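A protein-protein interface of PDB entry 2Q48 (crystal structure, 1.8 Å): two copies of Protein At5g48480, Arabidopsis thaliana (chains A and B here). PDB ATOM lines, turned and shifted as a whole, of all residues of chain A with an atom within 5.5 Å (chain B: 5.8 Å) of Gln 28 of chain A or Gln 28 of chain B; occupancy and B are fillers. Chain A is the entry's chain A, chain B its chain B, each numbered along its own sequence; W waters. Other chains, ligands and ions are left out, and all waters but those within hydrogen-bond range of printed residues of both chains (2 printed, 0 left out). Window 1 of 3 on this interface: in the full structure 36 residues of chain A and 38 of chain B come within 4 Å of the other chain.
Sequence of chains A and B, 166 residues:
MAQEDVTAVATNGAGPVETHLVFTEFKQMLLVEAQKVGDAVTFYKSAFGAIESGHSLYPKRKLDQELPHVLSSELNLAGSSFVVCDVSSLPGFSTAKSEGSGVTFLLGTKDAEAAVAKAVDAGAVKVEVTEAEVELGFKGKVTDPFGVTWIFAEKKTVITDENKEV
N of Met 29 of chain A sits at hydrogen-bond distance from O of Thr 104 of chain B. The backbone NH (N) of Met 29 of chain B is in hydrogen-bond range of the backbone carbonyl oxygen (O) of Thr 104 of chain A (2.8 Å). N of Leu 106 of chain A sits at hydrogen-bond distance from O of Lys 27 of chain B (2.7 Å). O of Lys 27 of chain A lies within hydrogen-bond range of N of Leu 106 of chain B (2.8 Å). The side-chain amide oxygen (OE1) of Gln 28 of chain B sits close to the side-chain amide oxygen (OE1) of Gln 28 of chain A, at 3.3 Å.
The backbone carbonyl oxygen (O) of Gln 28 of chain B is in hydrogen-bond range of the backbone NH (N) of Val 83 of chain B (2.9 Å). O of Gln 28 of chain A sits at hydrogen-bond distance from N of Val 83 of chain A.
Phe 26 of chain A touches Phe 82 of chain B. Phe 105 of chain B touches Phe 26 of chain A. Lys 27 of chain A touches Phe 105 of chain B (O to CA, 3.2 Å). CA of Gln 28 of chain A touches O of Thr 104 of chain B, at 3.7 Å. Gln 28 of chain A touches Phe 105 of chain B. Leu 106 of chain B touches Met 29 of chain A (CB to SD, 3.9 Å). Gln 28 of chain B touches Thr 104 of chain A (CG to O, 3.4 Å). Phe 26 of chain B touches Phe 105 of chain A (CE1 to CG, 3.6 Å). Lys 27 of chain B touches Phe 105 of chain A (O to CA, 3.6 Å). Phe 105 of chain A touches Gln 28 of chain B.
Gln 28 of chain A touches just these residues of chain B: Phe 26 (3.4 Å), Gln 28 (3.0 Å), Thr 104 (3.7 Å) and Phe 105 (3.5 Å). Gln 28 of chain B touches three residues of chain A. Of the printed residues of chain B, Lys 27 of chain A touches Phe 105 and Leu 106. Printed residues of chain B within 4 Å of Met 29 of chain A: Thr 104 (2.7 Å) and Leu 106 (3.9 Å). Of the printed residues of chain B, Thr 104 of chain A touches Gln 28 (3.4 Å) and Met 29 (2.8 Å). The nearest residue of chain B that does not touch Gln 28 of chain A is Ser 81 of chain B (4.1 Å).
Hydrophobic or aromatic side chains of chain A that line the printed part of chain B: Phe 26, Met 29, Phe 82, Phe 105 and Leu 106. Of the 13 printed residues of chain B, 9 touch a printed residue of chain A. Printed residues of chain B that touch a printed residue of chain A: Phe 26, Lys 27, Gln 28, Met 29, Ser 81, Phe 82, Thr 104, Phe 105 and Leu 106. Hydrophobic or aromatic side chains of chain B within 4 Å of the printed part of chain A: Phe 26, Met 29, Phe 82, Phe 105 and Leu 106.
Phe 26 of chain A touches Phe 82 of chain B, and with the chains exchanged Phe 82 of chain A touches Phe 26 of chain B. Lys 27 of chain A touches Phe 105 of chain B, and with the chains exchanged Phe 105 of chain A touches Lys 27 of chain B. Gln 28 of chain A touches its own counterpart, Gln 28 of chain B. Met 29 of chain A touches Leu 106 of chain B, and with the chains exchanged Leu 106 of chain A touches Met 29 of chain B. Positions printed for both chains: 26, 27, 28, 29, 30, 81, 82, 83, 103, 104, 105 and 106. Of the 21 pairs that touch across the chains among the printed residues, 19 have their exchanged pair printed and touching as well.
Water W1 lies within hydrogen-bond range of O of Ser 81 of chain B (2.6 Å), OE1 of Gln 28 of chain A (2.7 Å) and N of Gln 28 of chain B (2.9 Å). Water W2 lies within hydrogen-bond range of O of Met 29 of chain B, NE2 of Gln 28 of chain B and N of Thr 104 of chain A.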
ATOM      1  N   PHE A  26      20.600  -6.925  12.806  1.00  0.00           N
ATOM      2  CA  PHE A  26      21.290  -6.695  14.073  1.00  0.00           C
ATOM      3  C   PHE A  26      20.925  -5.315  14.607  1.00  0.00           C
ATOM      4  O   PHE A  26      21.274  -4.290  14.014  1.00  0.00           O
ATOM      5  CB  PHE A  26      22.805  -6.841  13.847  1.00  0.00           C
ATOM      6  CG  PHE A  26      23.690  -6.325  14.986  1.00  0.00           C
ATOM      7  CD1 PHE A  26      23.451  -6.672  16.337  1.00  0.00           C
ATOM      8  CD2 PHE A  26      24.794  -5.550  14.692  1.00  0.00           C
ATOM      9  CE1 PHE A  26      24.323  -6.238  17.348  1.00  0.00           C
ATOM     10  CE2 PHE A  26      25.668  -5.110  15.686  1.00  0.00           C
ATOM     11  CZ  PHE A  26      25.431  -5.453  17.026  1.00  0.00           C
ATOM     12  N   LYS A  27      20.208  -5.306  15.719  1.00  0.00           N
ATOM     13  CA  LYS A  27      19.770  -4.059  16.339  1.00  0.00           C
ATOM     14  C   LYS A  27      20.231  -3.979  17.780  1.00  0.00           C
ATOM     15  O   LYS A  27      20.394  -5.021  18.467  1.00  0.00           O
ATOM     16  CB  LYS A  27      18.250  -3.943  16.292  1.00  0.00           C
ATOM     17  CG  LYS A  27      17.683  -3.941  14.865  1.00  0.00           C
ATOM     18  CD  LYS A  27      16.167  -3.817  14.863  1.00  0.00           C
ATOM     19  CE  LYS A  27      15.502  -5.046  15.441  1.00  0.00           C
ATOM     20  NZ  LYS A  27      14.016  -5.021  15.203  1.00  0.00           N
ATOM     21  N   GLN A  28      20.429  -2.738  18.230  1.00  0.00           N
ATOM     22  CA  GLN A  28      20.893  -2.473  19.591  1.00  0.00           C
ATOM     23  C   GLN A  28      19.736  -1.879  20.320  1.00  0.00           C
ATOM     24  O   GLN A  28      19.160  -0.885  19.887  1.00  0.00           O
ATOM     25  CB  GLN A  28      22.092  -1.493  19.598  1.00  0.00           C
ATOM     26  CG  GLN A  28      21.983  -0.393  18.540  1.00  0.00           C
ATOM     27  CD  GLN A  28      23.351   0.261  18.170  1.00  0.00           C
ATOM     28  OE1 GLN A  28      24.339  -0.429  17.832  1.00  0.00           O
ATOM     29  NE2 GLN A  28      23.386   1.596  18.195  1.00  0.00           N
ATOM     30  N   MET A  29      19.413  -2.502  21.440  1.00  0.00           N
ATOM     31  CA  MET A  29      18.234  -2.152  22.217  1.00  0.00           C
ATOM     32  C   MET A  29      18.504  -1.376  23.462  1.00  0.00           C
ATOM     33  O   MET A  29      19.034  -1.937  24.438  1.00  0.00           O
ATOM     34  CB  MET A  29      17.543  -3.428  22.626  1.00  0.00           C
ATOM     35  CG  MET A  29      16.986  -4.184  21.447  1.00  0.00           C
ATOM     36  SD  MET A  29      16.749  -5.995  22.042  1.00  0.00           S
ATOM     37  CE  MET A  29      15.656  -5.693  23.738  1.00  0.00           C
ATOM     38  N   LEU A  30      18.038  -0.129  23.454  1.00  0.00           N
ATOM     39  CA  LEU A  30      18.240   0.767  24.573  1.00  0.00           C
ATOM     40  C   LEU A  30      17.018   0.582  25.503  1.00  0.00           C
ATOM     41  O   LEU A  30      15.912   1.073  25.202  1.00  0.00           O
ATOM     42  CB  LEU A  30      18.305   2.201  24.002  1.00  0.00           C
ATOM     43  CG  LEU A  30      18.810   3.268  24.956  1.00  0.00           C
ATOM     44  CD1 LEU A  30      19.035   4.608  24.255  1.00  0.00           C
ATOM     45  CD2 LEU A  30      17.774   3.370  26.038  1.00  0.00           C
ATOM     46  N   SER A  81      20.321   3.296  13.187  1.00  0.00           N
ATOM     47  CA  SER A  81      19.278   3.362  14.203  1.00  0.00           C
ATOM     48  C   SER A  81      19.504   2.558  15.450  1.00  0.00           C
ATOM     49  O   SER A  81      20.415   1.708  15.508  1.00  0.00           O
ATOM     50  CB  SER A  81      17.920   2.968  13.579  1.00  0.00           C
ATOM     51  OG  SER A  81      18.014   1.757  12.862  1.00  0.00           O
ATOM     52  N   PHE A  82      18.684   2.867  16.465  1.00  0.00           N
ATOM     53  CA  PHE A  82      18.687   2.085  17.734  1.00  0.00           C
ATOM     54  C   PHE A  82      17.220   1.932  18.085  1.00  0.00           C
ATOM     55  O   PHE A  82      16.354   2.592  17.463  1.00  0.00           O
ATOM     56  CB  PHE A  82      19.505   2.731  18.877  1.00  0.00           C
ATOM     57  CG  PHE A  82      19.102   4.140  19.267  1.00  0.00           C
ATOM     58  CD1 PHE A  82      19.476   5.234  18.486  1.00  0.00           C
ATOM     59  CD2 PHE A  82      18.438   4.384  20.476  1.00  0.00           C
ATOM     60  CE1 PHE A  82      19.191   6.549  18.909  1.00  0.00           C
ATOM     61  CE2 PHE A  82      18.166   5.696  20.889  1.00  0.00           C
ATOM     62  CZ  PHE A  82      18.540   6.746  20.104  1.00  0.00           C
ATOM     63  N   VAL A  83      16.921   1.070  19.056  1.00  0.00           N
ATOM     64  CA  VAL A  83      15.529   0.826  19.412  1.00  0.00           C
ATOM     65  C   VAL A  83      15.345   0.938  20.915  1.00  0.00           C
ATOM     66  O   VAL A  83      15.860   0.110  21.651  1.00  0.00           O
ATOM     67  CB  VAL A  83      15.081  -0.611  19.012  1.00  0.00           C
ATOM     68  CG1 VAL A  83      13.559  -0.767  19.247  1.00  0.00           C
ATOM     69  CG2 VAL A  83      15.481  -0.898  17.567  1.00  0.00           C
ATOM     70  N   VAL A 103      25.781   1.400  28.861  1.00  0.00           N
ATOM     71  CA  VAL A 103      25.359   1.783  27.529  1.00  0.00           C
ATOM     72  C   VAL A 103      26.026   3.072  27.103  1.00  0.00           C
ATOM     73  O   VAL A 103      25.817   4.120  27.704  1.00  0.00           O
ATOM     74  CB  VAL A 103      23.815   1.895  27.438  1.00  0.00           C
ATOM     75  CG1 VAL A 103      23.431   2.208  26.014  1.00  0.00           C
ATOM     76  CG2 VAL A 103      23.190   0.530  27.836  1.00  0.00           C
ATOM     77  N   THR A 104      26.772   2.962  26.006  1.00  0.00           N
ATOM     78  CA  THR A 104      27.593   4.064  25.510  1.00  0.00           C
ATOM     79  C   THR A 104      27.525   4.197  24.003  1.00  0.00           C
ATOM     80  O   THR A 104      27.765   3.237  23.270  1.00  0.00           O
ATOM     81  CB  THR A 104      29.058   3.770  25.872  1.00  0.00           C
ATOM     82  OG1 THR A 104      29.124   3.464  27.270  1.00  0.00           O
ATOM     83  CG2 THR A 104      29.923   4.988  25.574  1.00  0.00           C
ATOM     84  N   PHE A 105      27.210   5.405  23.540  1.00  0.00           N
ATOM     85  CA  PHE A 105      27.153   5.646  22.099  1.00  0.00           C
ATOM     86  C   PHE A 105      28.139   6.744  21.747  1.00  0.00           C
ATOM     87  O   PHE A 105      28.441   7.638  22.543  1.00  0.00           O
ATOM     88  CB  PHE A 105      25.756   6.152  21.659  1.00  0.00           C
ATOM     89  CG  PHE A 105      24.656   5.132  21.883  1.00  0.00           C
ATOM     90  CD1 PHE A 105      24.746   3.863  21.336  1.00  0.00           C
ATOM     91  CD2 PHE A 105      23.535   5.456  22.610  1.00  0.00           C
ATOM     92  CE1 PHE A 105      23.729   2.914  21.527  1.00  0.00           C
ATOM     93  CE2 PHE A 105      22.548   4.550  22.799  1.00  0.00           C
ATOM     94  CZ  PHE A 105      22.648   3.246  22.253  1.00  0.00           C
ATOM     95  N   LEU A 106      28.610   6.684  20.505  1.00  0.00           N
ATOM     96  CA  LEU A 106      29.525   7.684  19.983  1.00  0.00           C
ATOM     97  C   LEU A 106      28.800   8.462  18.876  1.00  0.00           C
ATOM     98  O   LEU A 106      28.122   7.827  18.055  1.00  0.00           O
ATOM     99  CB  LEU A 106      30.686   6.931  19.347  1.00  0.00           C
ATOM    100  CG  LEU A 106      31.695   7.652  18.525  1.00  0.00           C
ATOM    101  CD1 LEU A 106      32.957   6.702  18.462  1.00  0.00           C
ATOM    102  CD2 LEU A 106      31.165   7.903  17.111  1.00  0.00           C
ATOM    103  N   PHE B  26      27.192   7.431  14.090  1.00  0.00           N
ATOM    104  CA  PHE B  26      26.467   7.037  15.333  1.00  0.00           C
ATOM    105  C   PHE B  26      26.889   5.581  15.481  1.00  0.00           C
ATOM    106  O   PHE B  26      26.555   4.731  14.637  1.00  0.00           O
ATOM    107  CB  PHE B  26      24.927   7.100  15.137  1.00  0.00           C
ATOM    108  CG  PHE B  26      24.157   6.430  16.229  1.00  0.00           C
ATOM    109  CD1 PHE B  26      24.303   6.845  17.547  1.00  0.00           C
ATOM    110  CD2 PHE B  26      23.336   5.354  15.965  1.00  0.00           C
ATOM    111  CE1 PHE B  26      23.634   6.188  18.600  1.00  0.00           C
ATOM    112  CE2 PHE B  26      22.656   4.686  17.009  1.00  0.00           C
ATOM    113  CZ  PHE B  26      22.817   5.124  18.348  1.00  0.00           C
ATOM    114  N   LYS B  27      27.703   5.314  16.493  1.00  0.00           N
ATOM    115  CA  LYS B  27      28.247   3.971  16.746  1.00  0.00           C
ATOM    116  C   LYS B  27      28.167   3.569  18.244  1.00  0.00           C
ATOM    117  O   LYS B  27      28.605   4.342  19.103  1.00  0.00           O
ATOM    118  CB  LYS B  27      29.740   3.946  16.385  1.00  0.00           C
ATOM    119  CG  LYS B  27      30.035   4.346  14.913  1.00  0.00           C
ATOM    120  CD  LYS B  27      31.482   4.094  14.582  1.00  0.00           C
ATOM    121  CE  LYS B  27      31.801   4.427  13.151  1.00  0.00           C
ATOM    122  NZ  LYS B  27      31.145   3.474  12.217  1.00  0.00           N
ATOM    123  N   GLN B  28      27.628   2.391  18.538  1.00  0.00           N
ATOM    124  CA  GLN B  28      27.600   1.972  19.928  1.00  0.00           C
ATOM    125  C   GLN B  28      29.020   1.507  20.300  1.00  0.00           C
ATOM    126  O   GLN B  28      29.758   0.937  19.492  1.00  0.00           O
ATOM    127  CB  GLN B  28      26.637   0.813  20.185  1.00  0.00           C
ATOM    128  CG  GLN B  28      26.516   0.535  21.685  1.00  0.00           C
ATOM    129  CD  GLN B  28      25.266  -0.230  22.009  1.00  0.00           C
ATOM    130  OE1 GLN B  28      24.455  -0.514  21.107  1.00  0.00           O
ATOM    131  NE2 GLN B  28      25.072  -0.546  23.287  1.00  0.00           N
ATOM    132  N   MET B  29      29.368   1.749  21.553  1.00  0.00           N
ATOM    133  CA  MET B  29      30.666   1.367  22.102  1.00  0.00           C
ATOM    134  C   MET B  29      30.430   0.326  23.186  1.00  0.00           C
ATOM    135  O   MET B  29      29.730   0.602  24.184  1.00  0.00           O
ATOM    136  CB  MET B  29      31.354   2.601  22.718  1.00  0.00           C
ATOM    137  CG  MET B  29      31.754   3.613  21.648  1.00  0.00           C
ATOM    138  SD  MET B  29      32.408   5.278  22.380  1.00  0.00           S
ATOM    139  CE  MET B  29      33.603   4.327  23.773  1.00  0.00           C
ATOM    140  N   LEU B  30      30.982  -0.876  23.008  1.00  0.00           N
ATOM    141  CA  LEU B  30      30.828  -1.935  24.025  1.00  0.00           C
ATOM    142  C   LEU B  30      32.124  -1.887  24.863  1.00  0.00           C
ATOM    143  O   LEU B  30      33.242  -2.080  24.305  1.00  0.00           O
ATOM    144  CB  LEU B  30      30.734  -3.334  23.372  1.00  0.00           C
ATOM    145  CG  LEU B  30      30.886  -4.497  24.394  1.00  0.00           C
ATOM    146  CD1 LEU B  30      29.738  -4.464  25.414  1.00  0.00           C
ATOM    147  CD2 LEU B  30      30.928  -5.826  23.643  1.00  0.00           C
ATOM    148  N   SER B  81      26.877  -2.541  13.126  1.00  0.00           N
ATOM    149  CA  SER B  81      28.170  -2.774  13.692  1.00  0.00           C
ATOM    150  C   SER B  81      28.238  -2.176  15.076  1.00  0.00           C
ATOM    151  O   SER B  81      27.469  -1.289  15.401  1.00  0.00           O
ATOM    152  CB  SER B  81      29.203  -2.083  12.847  1.00  0.00           C
ATOM    153  OG  SER B  81      28.920  -0.721  12.690  1.00  0.00           O
ATOM    154  N   PHE B  82      29.209  -2.653  15.850  1.00  0.00           N
ATOM    155  CA  PHE B  82      29.432  -2.047  17.174  1.00  0.00           C
ATOM    156  C   PHE B  82      30.914  -2.042  17.421  1.00  0.00           C
ATOM    157  O   PHE B  82      31.653  -2.843  16.863  1.00  0.00           O
ATOM    158  CB  PHE B  82      28.692  -2.782  18.269  1.00  0.00           C
ATOM    159  CG  PHE B  82      29.060  -4.245  18.399  1.00  0.00           C
ATOM    160  CD1 PHE B  82      28.706  -5.179  17.410  1.00  0.00           C
ATOM    161  CD2 PHE B  82      29.764  -4.709  19.531  1.00  0.00           C
ATOM    162  CE1 PHE B  82      29.052  -6.535  17.548  1.00  0.00           C
ATOM    163  CE2 PHE B  82      30.100  -6.068  19.654  1.00  0.00           C
ATOM    164  CZ  PHE B  82      29.744  -6.970  18.662  1.00  0.00           C
ATOM    165  N   VAL B  83      31.375  -1.147  18.282  1.00  0.00           N
ATOM    166  CA  VAL B  83      32.802  -1.076  18.494  1.00  0.00           C
ATOM    167  C   VAL B  83      33.048  -1.671  19.865  1.00  0.00           C
ATOM    168  O   VAL B  83      32.248  -1.472  20.780  1.00  0.00           O
ATOM    169  CB  VAL B  83      33.257   0.339  18.474  1.00  0.00           C
ATOM    170  CG1 VAL B  83      32.545   1.109  17.272  1.00  0.00           C
ATOM    171  CG2 VAL B  83      32.968   0.989  19.774  1.00  0.00           C
ATOM    172  N   VAL B  84      34.154  -2.397  19.991  1.00  0.00           N
ATOM    173  CA  VAL B  84      34.514  -3.026  21.281  1.00  0.00           C
ATOM    174  C   VAL B  84      35.738  -2.329  21.827  1.00  0.00           C
ATOM    175  O   VAL B  84      36.735  -2.245  21.120  1.00  0.00           O
ATOM    176  CB  VAL B  84      34.951  -4.492  21.115  1.00  0.00           C
ATOM    177  CG1 VAL B  84      35.375  -5.056  22.558  1.00  0.00           C
ATOM    178  CG2 VAL B  84      33.826  -5.347  20.622  1.00  0.00           C
ATOM    179  N   VAL B 103      23.517  -3.740  28.264  1.00  0.00           N
ATOM    180  CA  VAL B 103      23.809  -3.810  26.821  1.00  0.00           C
ATOM    181  C   VAL B 103      23.042  -4.996  26.216  1.00  0.00           C
ATOM    182  O   VAL B 103      23.314  -6.161  26.557  1.00  0.00           O
ATOM    183  CB  VAL B 103      25.311  -3.939  26.581  1.00  0.00           C
ATOM    184  CG1 VAL B 103      25.599  -3.982  25.078  1.00  0.00           C
ATOM    185  CG2 VAL B 103      26.014  -2.708  27.163  1.00  0.00           C
ATOM    186  N   THR B 104      22.115  -4.651  25.325  1.00  0.00           N
ATOM    187  CA  THR B 104      21.186  -5.624  24.774  1.00  0.00           C
ATOM    188  C   THR B 104      21.096  -5.537  23.259  1.00  0.00           C
ATOM    189  O   THR B 104      20.898  -4.448  22.682  1.00  0.00           O
ATOM    190  CB  THR B 104      19.753  -5.352  25.416  1.00  0.00           C
ATOM    191  OG1 THR B 104      19.885  -5.275  26.836  1.00  0.00           O
ATOM    192  CG2 THR B 104      18.757  -6.451  25.061  1.00  0.00           C
ATOM    193  N   PHE B 105      21.249  -6.683  22.594  1.00  0.00           N
ATOM    194  CA  PHE B 105      21.127  -6.676  21.159  1.00  0.00           C
ATOM    195  C   PHE B 105      20.141  -7.708  20.695  1.00  0.00           C
ATOM    196  O   PHE B 105      19.915  -8.717  21.399  1.00  0.00           O
ATOM    197  CB  PHE B 105      22.453  -7.028  20.485  1.00  0.00           C
ATOM    198  CG  PHE B 105      23.566  -6.042  20.741  1.00  0.00           C
ATOM    199  CD1 PHE B 105      23.432  -4.687  20.426  1.00  0.00           C
ATOM    200  CD2 PHE B 105      24.743  -6.473  21.273  1.00  0.00           C
ATOM    201  CE1 PHE B 105      24.487  -3.780  20.668  1.00  0.00           C
ATOM    202  CE2 PHE B 105      25.798  -5.600  21.514  1.00  0.00           C
ATOM    203  CZ  PHE B 105      25.675  -4.250  21.214  1.00  0.00           C
ATOM    204  N   LEU B 106      19.549  -7.446  19.522  1.00  0.00           N
ATOM    205  CA  LEU B 106      18.640  -8.398  18.914  1.00  0.00           C
ATOM    206  C   LEU B 106      19.298  -8.864  17.614  1.00  0.00           C
ATOM    207  O   LEU B 106      19.935  -8.089  16.906  1.00  0.00           O
ATOM    208  CB  LEU B 106      17.289  -7.735  18.601  1.00  0.00           C
ATOM    209  CG  LEU B 106      16.120  -8.585  18.082  1.00  0.00           C
ATOM    210  CD1 LEU B 106      14.843  -7.798  18.382  1.00  0.00           C
ATOM    211  CD2 LEU B 106      16.236  -8.868  16.581  1.00  0.00           C
HETATM  212  O   HOH W   1      26.364   0.771  16.558  1.00  0.00           O
HETATM  213  O   HOH W   2      27.318   0.175  25.092  1.00  0.00           O
